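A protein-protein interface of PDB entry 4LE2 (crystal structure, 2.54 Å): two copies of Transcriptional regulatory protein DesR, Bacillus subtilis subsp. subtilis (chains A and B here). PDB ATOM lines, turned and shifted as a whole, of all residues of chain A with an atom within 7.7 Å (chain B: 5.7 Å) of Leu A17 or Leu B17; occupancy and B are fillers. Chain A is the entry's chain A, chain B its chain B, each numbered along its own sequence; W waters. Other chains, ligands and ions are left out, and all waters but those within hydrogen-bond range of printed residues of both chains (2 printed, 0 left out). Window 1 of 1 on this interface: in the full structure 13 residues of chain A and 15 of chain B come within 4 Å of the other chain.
The side-chain amide oxygen of Gln A14 lies close to the side-chain amide oxygen of Gln B14 (3.5 Å). N of Met A16 lies within hydrogen-bond range of O of Lys B106 (3.0 Å). The backbone carbonyl oxygen of Lys A106 sits at hydrogen-bond distance from the backbone NH of Gln B15 (3.4 Å). N of Met B16 is in hydrogen-bond range of O of Lys A106. The side-chain amide oxygen (OE1) of Gln B15 sits close to the backbone carbonyl oxygen (O) of Asp A107 (3.4 Å). The backbone carbonyl oxygen (O) of Ser A108 lies within hydrogen-bond range of the backbone NH (N) of Met B16, 3.1 Å away.
Water W1 lies within hydrogen-bond range of the backbone carbonyl oxygen (O) of Ala A20 (2.7 Å), the backbone carbonyl oxygen (O) of Ala B20 (2.7 Å) and the side-chain hydroxyl (OG) of Ser A23 (3.3 Å). Water W2 lies within hydrogen-bond range of the side-chain amide nitrogen (NE2) of Gln A14 and the side-chain amide nitrogen (NE2) of Gln B14.
Gln A15 touches Lys B106, and with the chains exchanged Lys A106 touches Gln B15. Met A16 touches Lys B106, and with the chains exchanged Lys A106 touches Met B16. Ala A20 touches Ser B110, and with the chains exchanged Ser A110 touches Ala B20. Leu A83 touches Met B16, but with the chains exchanged Met A16 does not touch Leu B83 (4.1 Å). Of the 23 pairs that touch across the chains among the printed residues, 17 have their exchanged pair printed and touching as well.
Printed residues of chain B that touch a printed residue of chain A: Gln B14, Gln B15, Met B16, Leu B17, Gly B19, Ala B20, Leu B21, Lys B106 and Ser B110. Of the 26 printed residues of chain A, 12 touch a printed residue of chain B. Among the printed residues, 23 pairs touch across the chains.
Among the printed residues, pairs that only touch across the chains: Gln A14 with Lys B106, Gln A15 with Lys B106, Gln A15 with Ser B110, Met A16 with Leu B21, Met A16 with Ser B110, Leu A17 with Leu B17, Gly A19 with Ser B110, Ala A20 with Ala B20, Ala A20 with Ser B110, Leu A83 with Met B16, Leu A105 with Met B16, Lys A106 with Gln B14, Ser A108 with Gln B15, Ser A110 with Gln B15, Ser A110 with Met B16, Ser A110 with Gly B19 and Ser A110 with Ala B20.
The backbone NH (N) of Gln A14 sits at hydrogen-bond distance from the side-chain carboxylate (OE2) of Glu A12, at 3.0 Å. The side-chain carboxylate (OE1) of Glu A12 lies within salt-bridge range of the side-chain amino group (NZ) of Lys A106. The side-chain amide oxygen (OE1) of Gln A14 is in hydrogen-bond range of the side-chain amino group (NZ) of Lys A106 (3.5 Å). The side-chain hydroxyl (OG) of Ser A108 is in hydrogen-bond range of the backbone carbonyl oxygen (O) of Leu A105 (2.7 Å). OE2 of Glu B12 lies close to N of Gln B14 (3.1 Å). The side-chain amino group (NZ) of Lys B106 lies within salt-bridge range of the side-chain carboxylate (OE1) of Glu B12, at 3.5 Å.
Of chain B, only Leu B17 comes within 4 Å of Leu A17. Leu B17 touches one residue of chain A. Printed residues of chain B within 4 Å of Leu A83: Met B16 (3.9 Å). Printed residues of chain A within 4 Å of Ala B20: Ala A20 (3.7 Å) and Ser A110 (3.7 Å). Leu A24 touches none of the printed residues of chain B. The nearest residue of chain B that does not touch Leu A17 is Met B16 (4.3 Å). The nearest printed residue of chain B that does not touch Ser A110 is Leu B18 (5.4 Å).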
ATOM      1  N   ILE A  10     -30.336 -12.094 -10.136  1.00  0.00           N
ATOM      2  CA  ILE A  10     -29.494 -11.814 -11.304  1.00  0.00           C
ATOM      3  C   ILE A  10     -29.776 -12.849 -12.393  1.00  0.00           C
ATOM      4  O   ILE A  10     -29.598 -14.031 -12.151  1.00  0.00           O
ATOM      5  CB  ILE A  10     -27.949 -11.718 -11.018  1.00  0.00           C
ATOM      6  CG1 ILE A  10     -27.628 -10.884  -9.771  1.00  0.00           C
ATOM      7  CG2 ILE A  10     -27.174 -11.199 -12.280  1.00  0.00           C
ATOM      8  CD1 ILE A  10     -26.173 -10.837  -9.388  1.00  0.00           C
ATOM      9  N   GLU A  12     -28.450 -13.753 -16.061  1.00  0.00           N
ATOM     10  CA  GLU A  12     -27.402 -13.539 -17.043  1.00  0.00           C
ATOM     11  C   GLU A  12     -27.024 -14.875 -17.677  1.00  0.00           C
ATOM     12  O   GLU A  12     -26.709 -15.814 -16.953  1.00  0.00           O
ATOM     13  CB  GLU A  12     -26.200 -12.830 -16.377  1.00  0.00           C
ATOM     14  CG  GLU A  12     -24.940 -12.742 -17.215  1.00  0.00           C
ATOM     15  CD  GLU A  12     -25.119 -11.972 -18.499  1.00  0.00           C
ATOM     16  OE1 GLU A  12     -25.068 -10.723 -18.445  1.00  0.00           O
ATOM     17  OE2 GLU A  12     -25.378 -12.608 -19.545  1.00  0.00           O
ATOM     18  N   ASP A  13     -27.068 -14.956 -19.035  1.00  0.00           N
ATOM     19  CA  ASP A  13     -26.719 -16.184 -19.766  1.00  0.00           C
ATOM     20  C   ASP A  13     -25.223 -16.468 -19.751  1.00  0.00           C
ATOM     21  O   ASP A  13     -24.860 -17.647 -19.740  1.00  0.00           O
ATOM     22  CB  ASP A  13     -27.295 -16.234 -21.196  1.00  0.00           C
ATOM     23  CG  ASP A  13     -26.915 -15.070 -22.109  1.00  0.00           C
ATOM     24  OD1 ASP A  13     -26.997 -13.884 -21.645  1.00  0.00           O
ATOM     25  OD2 ASP A  13     -26.620 -15.327 -23.315  1.00  0.00           O
ATOM     26  N   GLN A  14     -24.349 -15.420 -19.757  1.00  0.00           N
ATOM     27  CA  GLN A  14     -22.897 -15.663 -19.683  1.00  0.00           C
ATOM     28  C   GLN A  14     -22.463 -15.885 -18.245  1.00  0.00           C
ATOM     29  O   GLN A  14     -22.311 -14.943 -17.468  1.00  0.00           O
ATOM     30  CB  GLN A  14     -22.012 -14.699 -20.506  1.00  0.00           C
ATOM     31  CG  GLN A  14     -22.345 -13.208 -20.483  1.00  0.00           C
ATOM     32  CD  GLN A  14     -21.325 -12.381 -21.252  1.00  0.00           C
ATOM     33  OE1 GLN A  14     -20.844 -11.339 -20.778  1.00  0.00           O
ATOM     34  NE2 GLN A  14     -20.998 -12.798 -22.477  1.00  0.00           N
ATOM     35  N   GLN A  15     -22.380 -17.165 -17.881  1.00  0.00           N
ATOM     36  CA  GLN A  15     -22.071 -17.691 -16.550  1.00  0.00           C
ATOM     37  C   GLN A  15     -20.891 -17.074 -15.833  1.00  0.00           C
ATOM     38  O   GLN A  15     -20.900 -17.038 -14.594  1.00  0.00           O
ATOM     39  CB  GLN A  15     -21.910 -19.206 -16.587  1.00  0.00           C
ATOM     40  CG  GLN A  15     -23.207 -19.967 -16.780  1.00  0.00           C
ATOM     41  CD  GLN A  15     -23.093 -21.295 -16.111  1.00  0.00           C
ATOM     42  OE1 GLN A  15     -22.508 -22.255 -16.639  1.00  0.00           O
ATOM     43  NE2 GLN A  15     -23.520 -21.323 -14.874  1.00  0.00           N
ATOM     44  N   MET A  16     -19.868 -16.617 -16.582  1.00  0.00           N
ATOM     45  CA  MET A  16     -18.706 -15.997 -15.960  1.00  0.00           C
ATOM     46  C   MET A  16     -19.048 -14.671 -15.367  1.00  0.00           C
ATOM     47  O   MET A  16     -18.615 -14.406 -14.253  1.00  0.00           O
ATOM     48  CB  MET A  16     -17.496 -15.917 -16.876  1.00  0.00           C
ATOM     49  CG  MET A  16     -16.224 -15.831 -16.104  1.00  0.00           C
ATOM     50  SD  MET A  16     -14.886 -16.546 -17.016  1.00  0.00           S
ATOM     51  CE  MET A  16     -14.883 -18.226 -16.361  1.00  0.00           C
ATOM     52  N   LEU A  17     -19.878 -13.866 -16.056  1.00  0.00           N
ATOM     53  CA  LEU A  17     -20.350 -12.564 -15.549  1.00  0.00           C
ATOM     54  C   LEU A  17     -21.384 -12.777 -14.447  1.00  0.00           C
ATOM     55  O   LEU A  17     -21.336 -12.066 -13.444  1.00  0.00           O
ATOM     56  CB  LEU A  17     -20.879 -11.650 -16.681  1.00  0.00           C
ATOM     57  CG  LEU A  17     -21.324 -10.216 -16.295  1.00  0.00           C
ATOM     58  CD1 LEU A  17     -20.132  -9.325 -15.905  1.00  0.00           C
ATOM     59  CD2 LEU A  17     -22.110  -9.558 -17.425  1.00  0.00           C
ATOM     60  N   LEU A  18     -22.283 -13.787 -14.602  1.00  0.00           N
ATOM     61  CA  LEU A  18     -23.310 -14.151 -13.605  1.00  0.00           C
ATOM     62  C   LEU A  18     -22.696 -14.411 -12.226  1.00  0.00           C
ATOM     63  O   LEU A  18     -23.070 -13.758 -11.253  1.00  0.00           O
ATOM     64  CB  LEU A  18     -24.120 -15.376 -14.074  1.00  0.00           C
ATOM     65  CG  LEU A  18     -25.212 -15.932 -13.111  1.00  0.00           C
ATOM     66  CD1 LEU A  18     -26.294 -14.859 -12.768  1.00  0.00           C
ATOM     67  CD2 LEU A  18     -25.857 -17.160 -13.701  1.00  0.00           C
ATOM     68  N   GLY A  19     -21.723 -15.311 -12.176  1.00  0.00           N
ATOM     69  CA  GLY A  19     -21.018 -15.667 -10.954  1.00  0.00           C
ATOM     70  C   GLY A  19     -20.163 -14.547 -10.407  1.00  0.00           C
ATOM     71  O   GLY A  19     -20.152 -14.325  -9.192  1.00  0.00           O
ATOM     72  N   ALA A  20     -19.453 -13.811 -11.298  1.00  0.00           N
ATOM     73  CA  ALA A  20     -18.608 -12.678 -10.896  1.00  0.00           C
ATOM     74  C   ALA A  20     -19.441 -11.515 -10.313  1.00  0.00           C
ATOM     75  O   ALA A  20     -19.067 -10.979  -9.264  1.00  0.00           O
ATOM     76  CB  ALA A  20     -17.745 -12.216 -12.049  1.00  0.00           C
ATOM     77  N   LEU A  21     -20.597 -11.182 -10.934  1.00  0.00           N
ATOM     78  CA  LEU A  21     -21.490 -10.130 -10.405  1.00  0.00           C
ATOM     79  C   LEU A  21     -22.121 -10.540  -9.082  1.00  0.00           C
ATOM     80  O   LEU A  21     -22.256  -9.715  -8.187  1.00  0.00           O
ATOM     81  CB  LEU A  21     -22.604  -9.736 -11.379  1.00  0.00           C
ATOM     82  CG  LEU A  21     -22.227  -8.956 -12.632  1.00  0.00           C
ATOM     83  CD1 LEU A  21     -23.469  -8.641 -13.428  1.00  0.00           C
ATOM     84  CD2 LEU A  21     -21.405  -7.676 -12.302  1.00  0.00           C
ATOM     85  N   GLY A  22     -22.498 -11.809  -8.967  1.00  0.00           N
ATOM     86  CA  GLY A  22     -23.084 -12.348  -7.749  1.00  0.00           C
ATOM     87  C   GLY A  22     -22.130 -12.227  -6.581  1.00  0.00           C
ATOM     88  O   GLY A  22     -22.540 -11.821  -5.500  1.00  0.00           O
ATOM     89  N   SER A  23     -20.839 -12.524  -6.806  1.00  0.00           N
ATOM     90  CA  SER A  23     -19.777 -12.424  -5.801  1.00  0.00           C
ATOM     91  C   SER A  23     -19.570 -10.973  -5.375  1.00  0.00           C
ATOM     92  O   SER A  23     -19.480 -10.699  -4.178  1.00  0.00           O
ATOM     93  CB  SER A  23     -18.476 -13.019  -6.335  1.00  0.00           C
ATOM     94  OG  SER A  23     -17.320 -12.563  -5.646  1.00  0.00           O
ATOM     95  N   LEU A  24     -19.514 -10.053  -6.358  1.00  0.00           N
ATOM     96  CA  LEU A  24     -19.319  -8.611  -6.189  1.00  0.00           C
ATOM     97  C   LEU A  24     -20.436  -7.981  -5.350  1.00  0.00           C
ATOM     98  O   LEU A  24     -20.150  -7.312  -4.363  1.00  0.00           O
ATOM     99  CB  LEU A  24     -19.209  -7.937  -7.587  1.00  0.00           C
ATOM    100  CG  LEU A  24     -18.952  -6.421  -7.653  1.00  0.00           C
ATOM    101  CD1 LEU A  24     -17.531  -6.079  -7.262  1.00  0.00           C
ATOM    102  CD2 LEU A  24     -19.233  -5.898  -9.039  1.00  0.00           C
ATOM    103  N   LYS A  36     -30.087 -16.607  -8.717  1.00  0.00           N
ATOM    104  CA  LYS A  36     -29.368 -16.458 -10.001  1.00  0.00           C
ATOM    105  C   LYS A  36     -30.083 -17.279 -11.068  1.00  0.00           C
ATOM    106  O   LYS A  36     -30.659 -18.330 -10.745  1.00  0.00           O
ATOM    107  CB  LYS A  36     -27.895 -16.904  -9.865  1.00  0.00           C
ATOM    108  CG  LYS A  36     -27.015 -15.893  -9.119  1.00  0.00           C
ATOM    109  CD  LYS A  36     -25.523 -16.291  -9.095  1.00  0.00           C
ATOM    110  CE  LYS A  36     -25.135 -17.234  -7.988  1.00  0.00           C
ATOM    111  NZ  LYS A  36     -23.676 -17.523  -8.046  1.00  0.00           N
ATOM    112  N   ASP A  58     -29.892  -9.452 -18.251  1.00  0.00           N
ATOM    113  CA  ASP A  58     -29.260  -9.215 -19.547  1.00  0.00           C
ATOM    114  C   ASP A  58     -30.415  -9.039 -20.536  1.00  0.00           C
ATOM    115  O   ASP A  58     -31.371  -9.813 -20.483  1.00  0.00           O
ATOM    116  CB  ASP A  58     -28.361 -10.378 -20.001  1.00  0.00           C
ATOM    117  CG  ASP A  58     -27.406  -9.967 -21.113  1.00  0.00           C
ATOM    118  OD1 ASP A  58     -27.880  -9.494 -22.179  1.00  0.00           O
ATOM    119  OD2 ASP A  58     -26.203 -10.084 -20.920  1.00  0.00           O
ATOM    120  N   LEU A  83     -28.869  -4.964 -18.349  1.00  0.00           N
ATOM    121  CA  LEU A  83     -27.447  -5.020 -18.725  1.00  0.00           C
ATOM    122  C   LEU A  83     -27.385  -5.348 -20.192  1.00  0.00           C
ATOM    123  O   LEU A  83     -28.100  -6.244 -20.652  1.00  0.00           O
ATOM    124  CB  LEU A  83     -26.671  -6.090 -17.937  1.00  0.00           C
ATOM    125  CG  LEU A  83     -26.369  -5.795 -16.466  1.00  0.00           C
ATOM    126  CD1 LEU A  83     -25.304  -6.734 -15.961  1.00  0.00           C
ATOM    127  CD2 LEU A  83     -25.969  -4.325 -16.233  1.00  0.00           C
ATOM    128  N   THR A  84     -26.560  -4.622 -20.930  1.00  0.00           N
ATOM    129  CA  THR A  84     -26.432  -4.802 -22.381  1.00  0.00           C
ATOM    130  C   THR A  84     -25.000  -4.590 -22.845  1.00  0.00           C
ATOM    131  O   THR A  84     -24.302  -3.754 -22.302  1.00  0.00           O
ATOM    132  CB  THR A  84     -27.489  -3.936 -23.139  1.00  0.00           C
ATOM    133  OG1 THR A  84     -27.347  -4.129 -24.542  1.00  0.00           O
ATOM    134  CG2 THR A  84     -27.435  -2.429 -22.790  1.00  0.00           C
ATOM    135  N   THR A  85     -24.552  -5.377 -23.818  1.00  0.00           N
ATOM    136  CA  THR A  85     -23.213  -5.273 -24.430  1.00  0.00           C
ATOM    137  C   THR A  85     -23.208  -4.073 -25.347  1.00  0.00           C
ATOM    138  O   THR A  85     -22.263  -3.297 -25.301  1.00  0.00           O
ATOM    139  CB  THR A  85     -22.868  -6.562 -25.191  1.00  0.00           C
ATOM    140  OG1 THR A  85     -22.829  -7.647 -24.271  1.00  0.00           O
ATOM    141  CG2 THR A  85     -21.562  -6.485 -25.920  1.00  0.00           C
ATOM    142  N   LEU A 105     -24.607  -0.400 -19.553  1.00  0.00           N
ATOM    143  CA  LEU A 105     -23.735  -1.060 -20.515  1.00  0.00           C
ATOM    144  C   LEU A 105     -22.711  -1.895 -19.780  1.00  0.00           C
ATOM    145  O   LEU A 105     -22.278  -1.513 -18.695  1.00  0.00           O
ATOM    146  CB  LEU A 105     -23.022  -0.009 -21.362  1.00  0.00           C
ATOM    147  CG  LEU A 105     -23.554   0.211 -22.784  1.00  0.00           C
ATOM    148  CD1 LEU A 105     -25.069   0.422 -22.809  1.00  0.00           C
ATOM    149  CD2 LEU A 105     -22.927   1.410 -23.388  1.00  0.00           C
ATOM    150  N   LYS A 106     -22.306  -3.018 -20.371  1.00  0.00           N
ATOM    151  CA  LYS A 106     -21.286  -3.894 -19.801  1.00  0.00           C
ATOM    152  C   LYS A 106     -19.884  -3.273 -19.808  1.00  0.00           C
ATOM    153  O   LYS A 106     -18.980  -3.813 -19.182  1.00  0.00           O
ATOM    154  CB  LYS A 106     -21.310  -5.258 -20.468  1.00  0.00           C
ATOM    155  CG  LYS A 106     -22.538  -6.078 -20.079  1.00  0.00           C
ATOM    156  CD  LYS A 106     -22.576  -7.302 -20.918  1.00  0.00           C
ATOM    157  CE  LYS A 106     -23.717  -8.192 -20.575  1.00  0.00           C
ATOM    158  NZ  LYS A 106     -23.684  -9.406 -21.439  1.00  0.00           N
ATOM    159  N   ASP A 107     -19.715  -2.111 -20.469  1.00  0.00           N
ATOM    160  CA  ASP A 107     -18.469  -1.349 -20.493  1.00  0.00           C
ATOM    161  C   ASP A 107     -18.445  -0.301 -19.362  1.00  0.00           C
ATOM    162  O   ASP A 107     -17.466   0.420 -19.245  1.00  0.00           O
ATOM    163  CB  ASP A 107     -18.231  -0.707 -21.863  1.00  0.00           C
ATOM    164  N   SER A 108     -19.512  -0.215 -18.528  1.00  0.00           N
ATOM    165  CA  SER A 108     -19.589   0.713 -17.388  1.00  0.00           C
ATOM    166  C   SER A 108     -18.725   0.139 -16.238  1.00  0.00           C
ATOM    167  O   SER A 108     -18.645  -1.092 -16.099  1.00  0.00           O
ATOM    168  CB  SER A 108     -21.024   0.851 -16.882  1.00  0.00           C
ATOM    169  OG  SER A 108     -21.991   1.061 -17.904  1.00  0.00           O
ATOM    170  N   PRO A 109     -18.095   0.986 -15.388  1.00  0.00           N
ATOM    171  CA  PRO A 109     -17.292   0.442 -14.273  1.00  0.00           C
ATOM    172  C   PRO A 109     -18.140  -0.400 -13.310  1.00  0.00           C
ATOM    173  O   PRO A 109     -19.264  -0.014 -13.000  1.00  0.00           O
ATOM    174  CB  PRO A 109     -16.711   1.694 -13.604  1.00  0.00           C
ATOM    175  CG  PRO A 109     -16.834   2.783 -14.611  1.00  0.00           C
ATOM    176  CD  PRO A 109     -18.079   2.465 -15.383  1.00  0.00           C
ATOM    177  N   SER A 110     -17.626  -1.578 -12.885  1.00  0.00           N
ATOM    178  CA  SER A 110     -18.337  -2.481 -11.968  1.00  0.00           C
ATOM    179  C   SER A 110     -18.740  -1.796 -10.644  1.00  0.00           C
ATOM    180  O   SER A 110     -19.747  -2.167 -10.046  1.00  0.00           O
ATOM    181  CB  SER A 110     -17.519  -3.739 -11.699  1.00  0.00           C
ATOM    182  OG  SER A 110     -16.215  -3.427 -11.240  1.00  0.00           O
ATOM    183  N   LEU A 113     -22.234  -0.296 -10.445  1.00  0.00           N
ATOM    184  CA  LEU A 113     -23.378  -1.199 -10.377  1.00  0.00           C
ATOM    185  C   LEU A 113     -24.110  -1.155  -9.035  1.00  0.00           C
ATOM    186  O   LEU A 113     -25.332  -0.987  -9.040  1.00  0.00           O
ATOM    187  CB  LEU A 113     -23.061  -2.626 -10.848  1.00  0.00           C
ATOM    188  CG  LEU A 113     -24.244  -3.633 -10.865  1.00  0.00           C
ATOM    189  CD1 LEU A 113     -25.400  -3.160 -11.738  1.00  0.00           C
ATOM    190  CD2 LEU A 113     -23.789  -4.979 -11.281  1.00  0.00           C
ATOM    191  N   GLU B  12      -9.469  -6.731 -20.281  1.00  0.00           N
ATOM    192  CA  GLU B  12     -10.840  -6.922 -20.732  1.00  0.00           C
ATOM    193  C   GLU B  12     -11.423  -5.536 -21.041  1.00  0.00           C
ATOM    194  O   GLU B  12     -11.280  -4.621 -20.217  1.00  0.00           O
ATOM    195  CB  GLU B  12     -11.638  -7.663 -19.626  1.00  0.00           C
ATOM    196  CG  GLU B  12     -13.139  -7.771 -19.857  1.00  0.00           C
ATOM    197  CD  GLU B  12     -13.536  -8.497 -21.124  1.00  0.00           C
ATOM    198  OE1 GLU B  12     -13.304  -9.726 -21.204  1.00  0.00           O
ATOM    199  OE2 GLU B  12     -14.047  -7.830 -22.050  1.00  0.00           O
ATOM    200  N   GLN B  14     -14.750  -4.862 -21.660  1.00  0.00           N
ATOM    201  CA  GLN B  14     -16.002  -4.625 -20.946  1.00  0.00           C
ATOM    202  C   GLN B  14     -15.739  -4.491 -19.462  1.00  0.00           C
ATOM    203  O   GLN B  14     -15.544  -5.476 -18.752  1.00  0.00           O
ATOM    204  CB  GLN B  14     -17.194  -5.531 -21.347  1.00  0.00           C
ATOM    205  CG  GLN B  14     -16.938  -7.019 -21.576  1.00  0.00           C
ATOM    206  CD  GLN B  14     -18.214  -7.819 -21.831  1.00  0.00           C
ATOM    207  OE1 GLN B  14     -18.410  -8.909 -21.281  1.00  0.00           O
ATOM    208  NE2 GLN B  14     -19.122  -7.304 -22.665  1.00  0.00           N
ATOM    209  N   GLN B  15     -15.629  -3.235 -19.026  1.00  0.00           N
ATOM    210  CA  GLN B  15     -15.282  -2.807 -17.670  1.00  0.00           C
ATOM    211  C   GLN B  15     -16.044  -3.476 -16.530  1.00  0.00           C
ATOM    212  O   GLN B  15     -15.481  -3.615 -15.434  1.00  0.00           O
ATOM    213  CB  GLN B  15     -15.378  -1.289 -17.538  1.00  0.00           C
ATOM    214  CG  GLN B  15     -14.228  -0.547 -18.172  1.00  0.00           C
ATOM    215  CD  GLN B  15     -14.042   0.748 -17.456  1.00  0.00           C
ATOM    216  OE1 GLN B  15     -14.637   1.762 -17.815  1.00  0.00           O
ATOM    217  NE2 GLN B  15     -13.299   0.713 -16.355  1.00  0.00           N
ATOM    218  N   MET B  16     -17.312  -3.845 -16.761  1.00  0.00           N
ATOM    219  CA  MET B  16     -18.091  -4.504 -15.727  1.00  0.00           C
ATOM    220  C   MET B  16     -17.548  -5.892 -15.441  1.00  0.00           C
ATOM    221  O   MET B  16     -17.436  -6.235 -14.274  1.00  0.00           O
ATOM    222  CB  MET B  16     -19.568  -4.526 -16.067  1.00  0.00           C
ATOM    223  CG  MET B  16     -20.408  -4.594 -14.875  1.00  0.00           C
ATOM    224  SD  MET B  16     -22.101  -4.494 -15.394  1.00  0.00           S
ATOM    225  CE  MET B  16     -22.365  -2.710 -15.325  1.00  0.00           C
ATOM    226  N   LEU B  17     -17.155  -6.665 -16.483  1.00  0.00           N
ATOM    227  CA  LEU B  17     -16.549  -7.986 -16.305  1.00  0.00           C
ATOM    228  C   LEU B  17     -15.111  -7.843 -15.772  1.00  0.00           C
ATOM    229  O   LEU B  17     -14.712  -8.620 -14.903  1.00  0.00           O
ATOM    230  CB  LEU B  17     -16.595  -8.816 -17.608  1.00  0.00           C
ATOM    231  CG  LEU B  17     -16.030 -10.268 -17.560  1.00  0.00           C
ATOM    232  CD1 LEU B  17     -16.927 -11.208 -16.752  1.00  0.00           C
ATOM    233  CD2 LEU B  17     -15.844 -10.837 -18.963  1.00  0.00           C
ATOM    234  N   LEU B  18     -14.355  -6.825 -16.248  1.00  0.00           N
ATOM    235  CA  LEU B  18     -12.979  -6.553 -15.807  1.00  0.00           C
ATOM    236  C   LEU B  18     -12.893  -6.364 -14.286  1.00  0.00           C
ATOM    237  O   LEU B  18     -12.128  -7.067 -13.630  1.00  0.00           O
ATOM    238  CB  LEU B  18     -12.409  -5.330 -16.557  1.00  0.00           C
ATOM    239  CG  LEU B  18     -11.037  -4.808 -16.147  1.00  0.00           C
ATOM    240  CD1 LEU B  18      -9.960  -5.851 -16.374  1.00  0.00           C
ATOM    241  CD2 LEU B  18     -10.702  -3.549 -16.878  1.00  0.00           C
ATOM    242  N   GLY B  19     -13.707  -5.453 -13.750  1.00  0.00           N
ATOM    243  CA  GLY B  19     -13.767  -5.171 -12.321  1.00  0.00           C
ATOM    244  C   GLY B  19     -14.311  -6.331 -11.516  1.00  0.00           C
ATOM    245  O   GLY B  19     -13.764  -6.646 -10.455  1.00  0.00           O
ATOM    246  N   ALA B  20     -15.378  -6.996 -12.026  1.00  0.00           N
ATOM    247  CA  ALA B  20     -15.980  -8.162 -11.363  1.00  0.00           C
ATOM    248  C   ALA B  20     -14.999  -9.358 -11.294  1.00  0.00           C
ATOM    249  O   ALA B  20     -14.891  -9.982 -10.239  1.00  0.00           O
ATOM    250  CB  ALA B  20     -17.284  -8.560 -12.041  1.00  0.00           C
ATOM    251  N   LEU B  21     -14.252  -9.643 -12.385  1.00  0.00           N
ATOM    252  CA  LEU B  21     -13.260 -10.734 -12.384  1.00  0.00           C
ATOM    253  C   LEU B  21     -12.101 -10.428 -11.449  1.00  0.00           C
ATOM    254  O   LEU B  21     -11.621 -11.332 -10.774  1.00  0.00           O
ATOM    255  CB  LEU B  21     -12.715 -11.043 -13.794  1.00  0.00           C
ATOM    256  CG  LEU B  21     -13.636 -11.758 -14.777  1.00  0.00           C
ATOM    257  CD1 LEU B  21     -12.898 -12.055 -16.035  1.00  0.00           C
ATOM    258  CD2 LEU B  21     -14.222 -13.053 -14.204  1.00  0.00           C
ATOM    259  N   GLY B  22     -11.662  -9.167 -11.430  1.00  0.00           N
ATOM    260  CA  GLY B  22     -10.586  -8.711 -10.561  1.00  0.00           C
ATOM    261  C   GLY B  22     -10.924  -8.924  -9.104  1.00  0.00           C
ATOM    262  O   GLY B  22     -10.079  -9.397  -8.345  1.00  0.00           O
ATOM    263  N   ASP B  58      -9.079 -10.814 -23.115  1.00  0.00           N
ATOM    264  CA  ASP B  58     -10.187 -10.964 -24.053  1.00  0.00           C
ATOM    265  C   ASP B  58      -9.543 -11.028 -25.439  1.00  0.00           C
ATOM    266  O   ASP B  58      -8.682 -10.197 -25.734  1.00  0.00           O
ATOM    267  CB  ASP B  58     -11.175  -9.781 -24.000  1.00  0.00           C
ATOM    268  CG  ASP B  58     -12.522 -10.135 -24.604  1.00  0.00           C
ATOM    269  OD1 ASP B  58     -12.562 -10.530 -25.791  1.00  0.00           O
ATOM    270  OD2 ASP B  58     -13.525 -10.039 -23.893  1.00  0.00           O
ATOM    271  N   LEU B  83     -10.030 -15.286 -22.848  1.00  0.00           N
ATOM    272  CA  LEU B  83     -11.485 -15.207 -22.616  1.00  0.00           C
ATOM    273  C   LEU B  83     -12.156 -14.806 -23.908  1.00  0.00           C
ATOM    274  O   LEU B  83     -11.709 -13.874 -24.586  1.00  0.00           O
ATOM    275  CB  LEU B  83     -11.872 -14.183 -21.555  1.00  0.00           C
ATOM    276  CG  LEU B  83     -11.586 -14.542 -20.117  1.00  0.00           C
ATOM    277  CD1 LEU B  83     -12.383 -13.690 -19.218  1.00  0.00           C
ATOM    278  CD2 LEU B  83     -11.943 -15.994 -19.799  1.00  0.00           C
ATOM    279  N   LYS B 106     -16.870 -17.143 -22.106  1.00  0.00           N
ATOM    280  CA  LYS B 106     -17.555 -16.305 -21.123  1.00  0.00           C
ATOM    281  C   LYS B 106     -18.835 -16.954 -20.566  1.00  0.00           C
ATOM    282  O   LYS B 106     -19.387 -16.462 -19.586  1.00  0.00           O
ATOM    283  CB  LYS B 106     -17.826 -14.928 -21.715  1.00  0.00           C
ATOM    284  CG  LYS B 106     -16.569 -14.089 -21.801  1.00  0.00           C
ATOM    285  CD  LYS B 106     -16.858 -12.823 -22.525  1.00  0.00           C
ATOM    286  CE  LYS B 106     -15.649 -11.943 -22.595  1.00  0.00           C
ATOM    287  NZ  LYS B 106     -16.013 -10.654 -23.230  1.00  0.00           N
ATOM    288  N   SER B 110     -17.829 -19.195 -13.530  1.00  0.00           N
ATOM    289  CA  SER B 110     -16.755 -18.342 -12.981  1.00  0.00           C
ATOM    290  C   SER B 110     -15.785 -19.107 -12.043  1.00  0.00           C
ATOM    291  O   SER B 110     -14.619 -18.745 -11.957  1.00  0.00           O
ATOM    292  CB  SER B 110     -17.341 -17.108 -12.303  1.00  0.00           C
ATOM    293  OG  SER B 110     -18.289 -17.466 -11.311  1.00  0.00           O
HETATM  294  O   HOH W   1     -16.595 -10.700  -8.262  1.00  0.00           O
HETATM  295  O   HOH W   2     -20.239 -10.180 -24.079  1.00  0.00           O
